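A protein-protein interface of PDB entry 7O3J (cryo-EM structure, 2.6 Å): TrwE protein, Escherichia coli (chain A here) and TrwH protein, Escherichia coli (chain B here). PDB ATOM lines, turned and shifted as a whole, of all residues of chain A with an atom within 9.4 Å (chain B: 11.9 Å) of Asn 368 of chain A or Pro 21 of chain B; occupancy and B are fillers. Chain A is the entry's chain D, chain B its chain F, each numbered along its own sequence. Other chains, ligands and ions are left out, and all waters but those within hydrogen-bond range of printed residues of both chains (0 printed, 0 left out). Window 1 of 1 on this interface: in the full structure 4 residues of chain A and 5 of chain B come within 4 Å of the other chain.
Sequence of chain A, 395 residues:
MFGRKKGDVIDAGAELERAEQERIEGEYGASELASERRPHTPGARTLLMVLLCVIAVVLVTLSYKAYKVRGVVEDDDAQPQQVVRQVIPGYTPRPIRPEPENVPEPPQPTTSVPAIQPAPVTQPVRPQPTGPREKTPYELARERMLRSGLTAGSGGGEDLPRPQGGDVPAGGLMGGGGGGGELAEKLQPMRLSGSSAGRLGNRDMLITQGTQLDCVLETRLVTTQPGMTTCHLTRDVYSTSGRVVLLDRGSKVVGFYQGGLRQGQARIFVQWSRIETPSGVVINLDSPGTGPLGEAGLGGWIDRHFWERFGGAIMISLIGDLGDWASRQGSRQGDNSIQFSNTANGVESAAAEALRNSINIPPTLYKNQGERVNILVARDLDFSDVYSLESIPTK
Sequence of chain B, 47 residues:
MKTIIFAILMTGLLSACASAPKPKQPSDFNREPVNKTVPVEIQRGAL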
ATOM      1  N   VAL A 216      34.072   1.595  -7.338  1.00  0.00           N
ATOM      2  CA  VAL A 216      33.469   2.885  -7.030  1.00  0.00           C
ATOM      3  C   VAL A 216      33.754   3.839  -8.179  1.00  0.00           C
ATOM      4  O   VAL A 216      34.893   3.943  -8.640  1.00  0.00           O
ATOM      5  CB  VAL A 216      33.975   3.441  -5.687  1.00  0.00           C
ATOM      6  CG1 VAL A 216      35.473   3.582  -5.681  1.00  0.00           C
ATOM      7  CG2 VAL A 216      33.333   4.763  -5.391  1.00  0.00           C
ATOM      8  N   LEU A 217      32.719   4.514  -8.653  1.00  0.00           N
ATOM      9  CA  LEU A 217      32.857   5.380  -9.812  1.00  0.00           C
ATOM     10  C   LEU A 217      33.621   6.642  -9.449  1.00  0.00           C
ATOM     11  O   LEU A 217      33.250   7.359  -8.521  1.00  0.00           O
ATOM     12  CB  LEU A 217      31.485   5.741 -10.362  1.00  0.00           C
ATOM     13  CG  LEU A 217      31.458   6.367 -11.747  1.00  0.00           C
ATOM     14  CD1 LEU A 217      31.803   5.351 -12.802  1.00  0.00           C
ATOM     15  CD2 LEU A 217      30.099   6.962 -12.005  1.00  0.00           C
ATOM     16  N   GLU A 218      34.685   6.921 -10.194  1.00  0.00           N
ATOM     17  CA  GLU A 218      35.494   8.108  -9.966  1.00  0.00           C
ATOM     18  C   GLU A 218      34.958   9.324 -10.701  1.00  0.00           C
ATOM     19  O   GLU A 218      34.734  10.371 -10.094  1.00  0.00           O
ATOM     20  CB  GLU A 218      36.939   7.857 -10.400  1.00  0.00           C
ATOM     21  CG  GLU A 218      37.918   8.809  -9.766  1.00  0.00           C
ATOM     22  CD  GLU A 218      39.157   9.001 -10.601  1.00  0.00           C
ATOM     23  OE1 GLU A 218      39.153   8.560 -11.768  1.00  0.00           O
ATOM     24  OE2 GLU A 218      40.135   9.591 -10.095  1.00  0.00           O
ATOM     25  N   THR A 219      34.754   9.200 -12.002  1.00  0.00           N
ATOM     26  CA  THR A 219      34.289  10.310 -12.807  1.00  0.00           C
ATOM     27  C   THR A 219      32.788  10.501 -12.647  1.00  0.00           C
ATOM     28  O   THR A 219      32.035   9.559 -12.407  1.00  0.00           O
ATOM     29  CB  THR A 219      34.626  10.073 -14.275  1.00  0.00           C
ATOM     30  OG1 THR A 219      33.998   8.866 -14.716  1.00  0.00           O
ATOM     31  CG2 THR A 219      36.116   9.940 -14.454  1.00  0.00           C
ATOM     32  N   ARG A 220      32.359  11.747 -12.775  1.00  0.00           N
ATOM     33  CA  ARG A 220      30.947  12.070 -12.883  1.00  0.00           C
ATOM     34  C   ARG A 220      30.523  11.824 -14.321  1.00  0.00           C
ATOM     35  O   ARG A 220      31.259  12.161 -15.248  1.00  0.00           O
ATOM     36  CB  ARG A 220      30.708  13.520 -12.475  1.00  0.00           C
ATOM     37  CG  ARG A 220      29.381  14.081 -12.864  1.00  0.00           C
ATOM     38  CD  ARG A 220      29.049  15.247 -11.979  1.00  0.00           C
ATOM     39  NE  ARG A 220      27.698  15.739 -12.193  1.00  0.00           N
ATOM     40  CZ  ARG A 220      27.408  16.852 -12.852  1.00  0.00           C
ATOM     41  NH1 ARG A 220      28.379  17.589 -13.364  1.00  0.00           N
ATOM     42  NH2 ARG A 220      26.150  17.231 -12.996  1.00  0.00           N
ATOM     43  N   LEU A 221      29.364  11.215 -14.512  1.00  0.00           N
ATOM     44  CA  LEU A 221      28.976  10.720 -15.824  1.00  0.00           C
ATOM     45  C   LEU A 221      27.808  11.542 -16.359  1.00  0.00           C
ATOM     46  O   LEU A 221      26.758  11.620 -15.722  1.00  0.00           O
ATOM     47  CB  LEU A 221      28.620   9.238 -15.739  1.00  0.00           C
ATOM     48  CG  LEU A 221      28.490   8.412 -17.016  1.00  0.00           C
ATOM     49  CD1 LEU A 221      28.801   6.981 -16.698  1.00  0.00           C
ATOM     50  CD2 LEU A 221      27.120   8.502 -17.593  1.00  0.00           C
ATOM     51  N   VAL A 222      28.002  12.156 -17.524  1.00  0.00           N
ATOM     52  CA  VAL A 222      26.971  12.911 -18.226  1.00  0.00           C
ATOM     53  C   VAL A 222      27.003  12.463 -19.678  1.00  0.00           C
ATOM     54  O   VAL A 222      28.042  12.573 -20.334  1.00  0.00           O
ATOM     55  CB  VAL A 222      27.191  14.429 -18.122  1.00  0.00           C
ATOM     56  CG1 VAL A 222      26.132  15.168 -18.887  1.00  0.00           C
ATOM     57  CG2 VAL A 222      27.196  14.868 -16.678  1.00  0.00           C
ATOM     58  N   THR A 230      35.857   5.845 -15.427  1.00  0.00           N
ATOM     59  CA  THR A 230      36.940   5.309 -14.625  1.00  0.00           C
ATOM     60  C   THR A 230      36.401   4.950 -13.254  1.00  0.00           C
ATOM     61  O   THR A 230      35.612   5.699 -12.679  1.00  0.00           O
ATOM     62  CB  THR A 230      38.088   6.310 -14.497  1.00  0.00           C
ATOM     63  OG1 THR A 230      38.601   6.608 -15.796  1.00  0.00           O
ATOM     64  CG2 THR A 230      39.201   5.748 -13.654  1.00  0.00           C
ATOM     65  N   LEU A 298      24.464   1.720 -16.479  1.00  0.00           N
ATOM     66  CA  LEU A 298      24.513   2.695 -15.403  1.00  0.00           C
ATOM     67  C   LEU A 298      23.315   3.623 -15.505  1.00  0.00           C
ATOM     68  O   LEU A 298      22.929   4.040 -16.596  1.00  0.00           O
ATOM     69  CB  LEU A 298      25.811   3.496 -15.459  1.00  0.00           C
ATOM     70  CG  LEU A 298      26.976   2.987 -14.617  1.00  0.00           C
ATOM     71  CD1 LEU A 298      27.419   1.631 -15.068  1.00  0.00           C
ATOM     72  CD2 LEU A 298      28.124   3.949 -14.730  1.00  0.00           C
ATOM     73  N   GLY A 299      22.721   3.931 -14.367  1.00  0.00           N
ATOM     74  CA  GLY A 299      21.560   4.793 -14.333  1.00  0.00           C
ATOM     75  C   GLY A 299      21.696   5.827 -13.242  1.00  0.00           C
ATOM     76  O   GLY A 299      22.286   5.579 -12.192  1.00  0.00           O
ATOM     77  N   GLY A 300      21.142   6.993 -13.501  1.00  0.00           N
ATOM     78  CA  GLY A 300      21.149   8.084 -12.537  1.00  0.00           C
ATOM     79  C   GLY A 300      19.926   8.931 -12.696  1.00  0.00           C
ATOM     80  O   GLY A 300      18.824   8.410 -12.908  1.00  0.00           O
ATOM     81  N   TRP A 301      20.103  10.239 -12.597  1.00  0.00           N
ATOM     82  CA  TRP A 301      19.018  11.190 -12.764  1.00  0.00           C
ATOM     83  C   TRP A 301      18.887  11.541 -14.239  1.00  0.00           C
ATOM     84  O   TRP A 301      19.889  11.784 -14.910  1.00  0.00           O
ATOM     85  CB  TRP A 301      19.293  12.434 -11.925  1.00  0.00           C
ATOM     86  CG  TRP A 301      18.270  13.488 -12.033  1.00  0.00           C
ATOM     87  CD1 TRP A 301      17.114  13.575 -11.334  1.00  0.00           C
ATOM     88  CD2 TRP A 301      18.310  14.628 -12.890  1.00  0.00           C
ATOM     89  NE1 TRP A 301      16.424  14.695 -11.704  1.00  0.00           N
ATOM     90  CE2 TRP A 301      17.140  15.358 -12.661  1.00  0.00           C
ATOM     91  CE3 TRP A 301      19.223  15.097 -13.832  1.00  0.00           C
ATOM     92  CZ2 TRP A 301      16.857  16.529 -13.338  1.00  0.00           C
ATOM     93  CZ3 TRP A 301      18.940  16.256 -14.501  1.00  0.00           C
ATOM     94  CH2 TRP A 301      17.768  16.961 -14.254  1.00  0.00           C
ATOM     95  N   ILE A 302      17.659  11.563 -14.742  1.00  0.00           N
ATOM     96  CA  ILE A 302      17.395  11.747 -16.163  1.00  0.00           C
ATOM     97  C   ILE A 302      16.801  13.127 -16.387  1.00  0.00           C
ATOM     98  O   ILE A 302      15.825  13.505 -15.733  1.00  0.00           O
ATOM     99  CB  ILE A 302      16.455  10.662 -16.708  1.00  0.00           C
ATOM    100  CG1 ILE A 302      17.053   9.288 -16.468  1.00  0.00           C
ATOM    101  CG2 ILE A 302      16.229  10.862 -18.184  1.00  0.00           C
ATOM    102  CD1 ILE A 302      18.099   8.927 -17.457  1.00  0.00           C
ATOM    103  N   ASP A 303      17.389  13.872 -17.313  1.00  0.00           N
ATOM    104  CA  ASP A 303      16.867  15.157 -17.752  1.00  0.00           C
ATOM    105  C   ASP A 303      16.160  14.934 -19.078  1.00  0.00           C
ATOM    106  O   ASP A 303      16.799  14.607 -20.079  1.00  0.00           O
ATOM    107  CB  ASP A 303      17.992  16.176 -17.894  1.00  0.00           C
ATOM    108  CG  ASP A 303      17.505  17.527 -18.353  1.00  0.00           C
ATOM    109  OD1 ASP A 303      18.337  18.328 -18.813  1.00  0.00           O
ATOM    110  OD2 ASP A 303      16.295  17.799 -18.248  1.00  0.00           O
ATOM    111  N   THR A 364      19.049  13.071 -21.243  1.00  0.00           N
ATOM    112  CA  THR A 364      20.420  13.088 -20.763  1.00  0.00           C
ATOM    113  C   THR A 364      20.477  12.477 -19.372  1.00  0.00           C
ATOM    114  O   THR A 364      19.650  12.788 -18.516  1.00  0.00           O
ATOM    115  CB  THR A 364      20.975  14.512 -20.729  1.00  0.00           C
ATOM    116  OG1 THR A 364      20.934  15.068 -22.043  1.00  0.00           O
ATOM    117  CG2 THR A 364      22.401  14.518 -20.254  1.00  0.00           C
ATOM    118  N   LEU A 365      21.454  11.610 -19.153  1.00  0.00           N
ATOM    119  CA  LEU A 365      21.639  10.940 -17.879  1.00  0.00           C
ATOM    120  C   LEU A 365      22.752  11.608 -17.092  1.00  0.00           C
ATOM    121  O   LEU A 365      23.807  11.927 -17.641  1.00  0.00           O
ATOM    122  CB  LEU A 365      21.969   9.466 -18.090  1.00  0.00           C
ATOM    123  CG  LEU A 365      22.037   8.555 -16.875  1.00  0.00           C
ATOM    124  CD1 LEU A 365      21.321   7.291 -17.192  1.00  0.00           C
ATOM    125  CD2 LEU A 365      23.469   8.253 -16.533  1.00  0.00           C
ATOM    126  N   TYR A 366      22.507  11.827 -15.808  1.00  0.00           N
ATOM    127  CA  TYR A 366      23.496  12.374 -14.891  1.00  0.00           C
ATOM    128  C   TYR A 366      23.726  11.363 -13.787  1.00  0.00           C
ATOM    129  O   TYR A 366      22.778  10.948 -13.120  1.00  0.00           O
ATOM    130  CB  TYR A 366      23.026  13.699 -14.296  1.00  0.00           C
ATOM    131  CG  TYR A 366      22.976  14.836 -15.273  1.00  0.00           C
ATOM    132  CD1 TYR A 366      21.918  14.973 -16.148  1.00  0.00           C
ATOM    133  CD2 TYR A 366      23.975  15.784 -15.307  1.00  0.00           C
ATOM    134  CE1 TYR A 366      21.866  16.004 -17.035  1.00  0.00           C
ATOM    135  CE2 TYR A 366      23.927  16.824 -16.191  1.00  0.00           C
ATOM    136  CZ  TYR A 366      22.871  16.927 -17.053  1.00  0.00           C
ATOM    137  OH  TYR A 366      22.818  17.967 -17.942  1.00  0.00           O
ATOM    138  N   LYS A 367      24.976  10.971 -13.586  1.00  0.00           N
ATOM    139  CA  LYS A 367      25.344  10.077 -12.503  1.00  0.00           C
ATOM    140  C   LYS A 367      26.439  10.728 -11.680  1.00  0.00           C
ATOM    141  O   LYS A 367      27.451  11.163 -12.229  1.00  0.00           O
ATOM    142  CB  LYS A 367      25.809   8.726 -13.030  1.00  0.00           C
ATOM    143  CG  LYS A 367      25.838   7.665 -11.971  1.00  0.00           C
ATOM    144  CD  LYS A 367      26.097   6.313 -12.556  1.00  0.00           C
ATOM    145  CE  LYS A 367      26.206   5.290 -11.462  1.00  0.00           C
ATOM    146  NZ  LYS A 367      25.055   5.390 -10.541  1.00  0.00           N
ATOM    147  N   ASN A 368      26.235  10.788 -10.373  1.00  0.00           N
ATOM    148  CA  ASN A 368      27.170  11.480  -9.509  1.00  0.00           C
ATOM    149  C   ASN A 368      28.459  10.688  -9.353  1.00  0.00           C
ATOM    150  O   ASN A 368      28.509   9.476  -9.555  1.00  0.00           O
ATOM    151  CB  ASN A 368      26.550  11.724  -8.140  1.00  0.00           C
ATOM    152  CG  ASN A 368      25.720  12.970  -8.103  1.00  0.00           C
ATOM    153  OD1 ASN A 368      26.079  13.982  -8.693  1.00  0.00           O
ATOM    154  ND2 ASN A 368      24.595  12.907  -7.412  1.00  0.00           N
ATOM    155  N   GLN A 369      29.517  11.399  -8.997  1.00  0.00           N
ATOM    156  CA  GLN A 369      30.791  10.775  -8.707  1.00  0.00           C
ATOM    157  C   GLN A 369      30.737  10.076  -7.355  1.00  0.00           C
ATOM    158  O   GLN A 369      30.008  10.485  -6.449  1.00  0.00           O
ATOM    159  CB  GLN A 369      31.902  11.822  -8.725  1.00  0.00           C
ATOM    160  CG  GLN A 369      32.030  12.605  -7.440  1.00  0.00           C
ATOM    161  CD  GLN A 369      31.293  13.917  -7.472  1.00  0.00           C
ATOM    162  OE1 GLN A 369      30.441  14.141  -8.323  1.00  0.00           O
ATOM    163  NE2 GLN A 369      31.615  14.792  -6.539  1.00  0.00           N
ATOM    164  N   GLY A 370      31.510   9.003  -7.229  1.00  0.00           N
ATOM    165  CA  GLY A 370      31.542   8.249  -5.997  1.00  0.00           C
ATOM    166  C   GLY A 370      30.469   7.199  -5.862  1.00  0.00           C
ATOM    167  O   GLY A 370      30.333   6.617  -4.783  1.00  0.00           O
ATOM    168  N   GLU A 371      29.712   6.931  -6.915  1.00  0.00           N
ATOM    169  CA  GLU A 371      28.645   5.949  -6.855  1.00  0.00           C
ATOM    170  C   GLU A 371      29.195   4.544  -7.037  1.00  0.00           C
ATOM    171  O   GLU A 371      30.155   4.328  -7.773  1.00  0.00           O
ATOM    172  CB  GLU A 371      27.597   6.237  -7.923  1.00  0.00           C
ATOM    173  CG  GLU A 371      26.848   7.528  -7.713  1.00  0.00           C
ATOM    174  CD  GLU A 371      25.979   7.506  -6.477  1.00  0.00           C
ATOM    175  OE1 GLU A 371      25.472   6.423  -6.117  1.00  0.00           O
ATOM    176  OE2 GLU A 371      25.809   8.575  -5.854  1.00  0.00           O
ATOM    177  N   ARG A 372      28.569   3.588  -6.364  1.00  0.00           N
ATOM    178  CA  ARG A 372      28.985   2.199  -6.454  1.00  0.00           C
ATOM    179  C   ARG A 372      28.454   1.559  -7.730  1.00  0.00           C
ATOM    180  O   ARG A 372      27.300   1.759  -8.106  1.00  0.00           O
ATOM    181  CB  ARG A 372      28.477   1.432  -5.241  1.00  0.00           C
ATOM    182  CG  ARG A 372      29.427   0.398  -4.716  1.00  0.00           C
ATOM    183  CD  ARG A 372      28.737  -0.468  -3.691  1.00  0.00           C
ATOM    184  NE  ARG A 372      28.707   0.163  -2.379  1.00  0.00           N
ATOM    185  CZ  ARG A 372      29.590  -0.077  -1.420  1.00  0.00           C
ATOM    186  NH1 ARG A 372      29.489   0.541  -0.257  1.00  0.00           N
ATOM    187  NH2 ARG A 372      30.570  -0.941  -1.626  1.00  0.00           N
ATOM    188  N   VAL A 373      29.307   0.784  -8.400  1.00  0.00           N
ATOM    189  CA  VAL A 373      28.930   0.073  -9.613  1.00  0.00           C
ATOM    190  C   VAL A 373      29.544  -1.321  -9.577  1.00  0.00           C
ATOM    191  O   VAL A 373      30.464  -1.598  -8.809  1.00  0.00           O
ATOM    192  CB  VAL A 373      29.371   0.823 -10.886  1.00  0.00           C
ATOM    193  CG1 VAL A 373      28.535   2.061 -11.085  1.00  0.00           C
ATOM    194  CG2 VAL A 373      30.809   1.206 -10.797  1.00  0.00           C
ATOM    195  N   CYS B  17      13.526  24.030 -15.071  1.00  0.00           N
ATOM    196  CA  CYS B  17      12.989  24.130 -13.719  1.00  0.00           C
ATOM    197  C   CYS B  17      13.501  22.992 -12.842  1.00  0.00           C
ATOM    198  O   CYS B  17      13.308  22.997 -11.628  1.00  0.00           O
ATOM    199  CB  CYS B  17      11.460  24.127 -13.750  1.00  0.00           C
ATOM    200  SG  CYS B  17      10.686  24.905 -12.316  1.00  0.00           S
ATOM    201  N   ALA B  18      14.152  22.016 -13.469  1.00  0.00           N
ATOM    202  CA  ALA B  18      14.732  20.875 -12.773  1.00  0.00           C
ATOM    203  C   ALA B  18      16.206  20.771 -13.134  1.00  0.00           C
ATOM    204  O   ALA B  18      16.567  20.854 -14.313  1.00  0.00           O
ATOM    205  CB  ALA B  18      14.005  19.579 -13.130  1.00  0.00           C
ATOM    206  N   SER B  19      17.050  20.591 -12.123  1.00  0.00           N
ATOM    207  CA  SER B  19      18.486  20.491 -12.308  1.00  0.00           C
ATOM    208  C   SER B  19      18.999  19.203 -11.683  1.00  0.00           C
ATOM    209  O   SER B  19      18.333  18.584 -10.851  1.00  0.00           O
ATOM    210  CB  SER B  19      19.208  21.695 -11.700  1.00  0.00           C
ATOM    211  OG  SER B  19      20.612  21.535 -11.780  1.00  0.00           O
ATOM    212  N   ALA B  20      20.190  18.802 -12.101  1.00  0.00           N
ATOM    213  CA  ALA B  20      20.775  17.563 -11.610  1.00  0.00           C
ATOM    214  C   ALA B  20      21.070  17.678 -10.121  1.00  0.00           C
ATOM    215  O   ALA B  20      21.697  18.653  -9.694  1.00  0.00           O
ATOM    216  CB  ALA B  20      22.050  17.242 -12.376  1.00  0.00           C
ATOM    217  N   PRO B  21      20.635  16.723  -9.305  1.00  0.00           N
ATOM    218  CA  PRO B  21      20.886  16.820  -7.865  1.00  0.00           C
ATOM    219  C   PRO B  21      22.368  16.732  -7.547  1.00  0.00           C
ATOM    220  O   PRO B  21      23.132  16.048  -8.229  1.00  0.00           O
ATOM    221  CB  PRO B  21      20.118  15.627  -7.291  1.00  0.00           C
ATOM    222  CG  PRO B  21      20.004  14.682  -8.412  1.00  0.00           C
ATOM    223  CD  PRO B  21      19.889  15.508  -9.651  1.00  0.00           C
ATOM    224  N   LYS B  22      22.767  17.437  -6.509  1.00  0.00           N
ATOM    225  CA  LYS B  22      24.138  17.430  -6.043  1.00  0.00           C
ATOM    226  C   LYS B  22      24.393  16.202  -5.174  1.00  0.00           C
ATOM    227  O   LYS B  22      23.466  15.653  -4.581  1.00  0.00           O
ATOM    228  CB  LYS B  22      24.426  18.689  -5.239  1.00  0.00           C
ATOM    229  CG  LYS B  22      24.243  19.976  -6.006  1.00  0.00           C
ATOM    230  CD  LYS B  22      25.311  20.140  -7.063  1.00  0.00           C
ATOM    231  CE  LYS B  22      26.655  20.454  -6.436  1.00  0.00           C
ATOM    232  NZ  LYS B  22      27.682  20.750  -7.466  1.00  0.00           N
ATOM    233  N   PRO B  23      25.640  15.753  -5.085  1.00  0.00           N
ATOM    234  CA  PRO B  23      25.969  14.701  -4.123  1.00  0.00           C
ATOM    235  C   PRO B  23      25.843  15.222  -2.703  1.00  0.00           C
ATOM    236  O   PRO B  23      25.905  16.426  -2.446  1.00  0.00           O
ATOM    237  CB  PRO B  23      27.421  14.346  -4.459  1.00  0.00           C
ATOM    238  CG  PRO B  23      27.666  14.923  -5.792  1.00  0.00           C
ATOM    239  CD  PRO B  23      26.803  16.126  -5.899  1.00  0.00           C
ATOM    240  N   LYS B  24      25.652  14.293  -1.775  1.00  0.00           N
ATOM    241  CA  LYS B  24      25.441  14.665  -0.385  1.00  0.00           C
ATOM    242  C   LYS B  24      26.623  15.459   0.152  1.00  0.00           C
ATOM    243  O   LYS B  24      27.780  15.077  -0.035  1.00  0.00           O
ATOM    244  CB  LYS B  24      25.221  13.419   0.468  1.00  0.00           C
ATOM    245  CG  LYS B  24      25.484  13.649   1.942  1.00  0.00           C
ATOM    246  CD  LYS B  24      25.659  12.352   2.694  1.00  0.00           C
ATOM    247  CE  LYS B  24      24.382  11.549   2.687  1.00  0.00           C
ATOM    248  NZ  LYS B  24      24.400  10.497   3.736  1.00  0.00           N
ATOM    249  N   GLN B  25      26.328  16.561   0.805  1.00  0.00           N
ATOM    250  CA  GLN B  25      27.332  17.340   1.516  1.00  0.00           C
ATOM    251  C   GLN B  25      27.448  16.835   2.946  1.00  0.00           C
ATOM    252  O   GLN B  25      26.435  16.750   3.648  1.00  0.00           O
ATOM    253  CB  GLN B  25      26.965  18.814   1.524  1.00  0.00           C
ATOM    254  CG  GLN B  25      27.342  19.561   0.265  1.00  0.00           C
ATOM    255  CD  GLN B  25      28.836  19.578   0.023  1.00  0.00           C
ATOM    256  OE1 GLN B  25      29.308  19.185  -1.042  1.00  0.00           O
ATOM    257  NE2 GLN B  25      29.590  20.033   1.015  1.00  0.00           N
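Of the 9 printed residues of chain B, 5 touch a printed residue of chain A. Hydrophobic or aromatic side chains of chain B within 4 Å of the printed part of chain A: Ala 20, Pro 21 and Pro 23. Of the 24 printed residues of chain A, 4 touch a printed residue of chain B. Printed residues of chain A that touch a printed residue of chain B: Trp 301, Tyr 366, Asn 368 and Gln 369. Hydrophobic or aromatic side chains of chain A within 4 Å of the printed part of chain B: Trp 301 and Tyr 366.
Among the printed residues, pairs that only touch across the chains: Asn 368 of chain A with Pro 23 of chain B, Trp 301 of chain A with Pro 21 of chain B, Trp 301 of chain A with Ser 19 of chain B, Asn 368 of chain A with Pro 21 of chain B, Trp 301 of chain A with Ala 20 of chain B, Tyr 366 of chain A with Ala 20 of chain B, Gln 369 of chain A with Pro 23 of chain B and Asn 368 of chain A with Lys 22 of chain B.
No residue of chain B comes within 4 Å of Leu 217 of chain A. No residue of chain B comes within 4 Å of Leu 221 of chain A. Val 222 of chain A touches none of the printed residues of chain B. No residue of chain B comes within 4 Å of Gly 300 of chain A. No residue of chain B comes within 4 Å of Lys 367 of chain A. Of the printed residues of chain B, Asn 368 of chain A touches Pro 21, Lys 22 and Pro 23. Of chain B, only Pro 23 comes within 4 Å of Gln 369 of chain A. No residue of chain B comes within 4 Å of Glu 371 of chain A. Cys 17 of chain B touches none of the printed residues of chain A. Printed residues of chain A within 4 Å of Ala 20 of chain B: Trp 301 and Tyr 366. Pro 21 of chain B touches just these residues of chain A: Trp 301 (3.5 Å) and Asn 368 (3.6 Å). Printed residues of chain A within 4 Å of Lys 22 of chain B: Asn 368. Of the printed residues of chain A, Pro 23 of chain B touches Asn 368 and Gln 369. The nearest printed residue of chain B that does not touch Asn 368 of chain A is Lys 24 of chain B (5.9 Å). The nearest residue of chain A that does not touch Pro 21 of chain B is Arg 220 of chain A (5.8 Å).
The backbone NH (N) of Tyr 366 of chain A sits at hydrogen-bond distance from the backbone carbonyl oxygen (O) of Trp 301 of chain A (2.8 Å).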
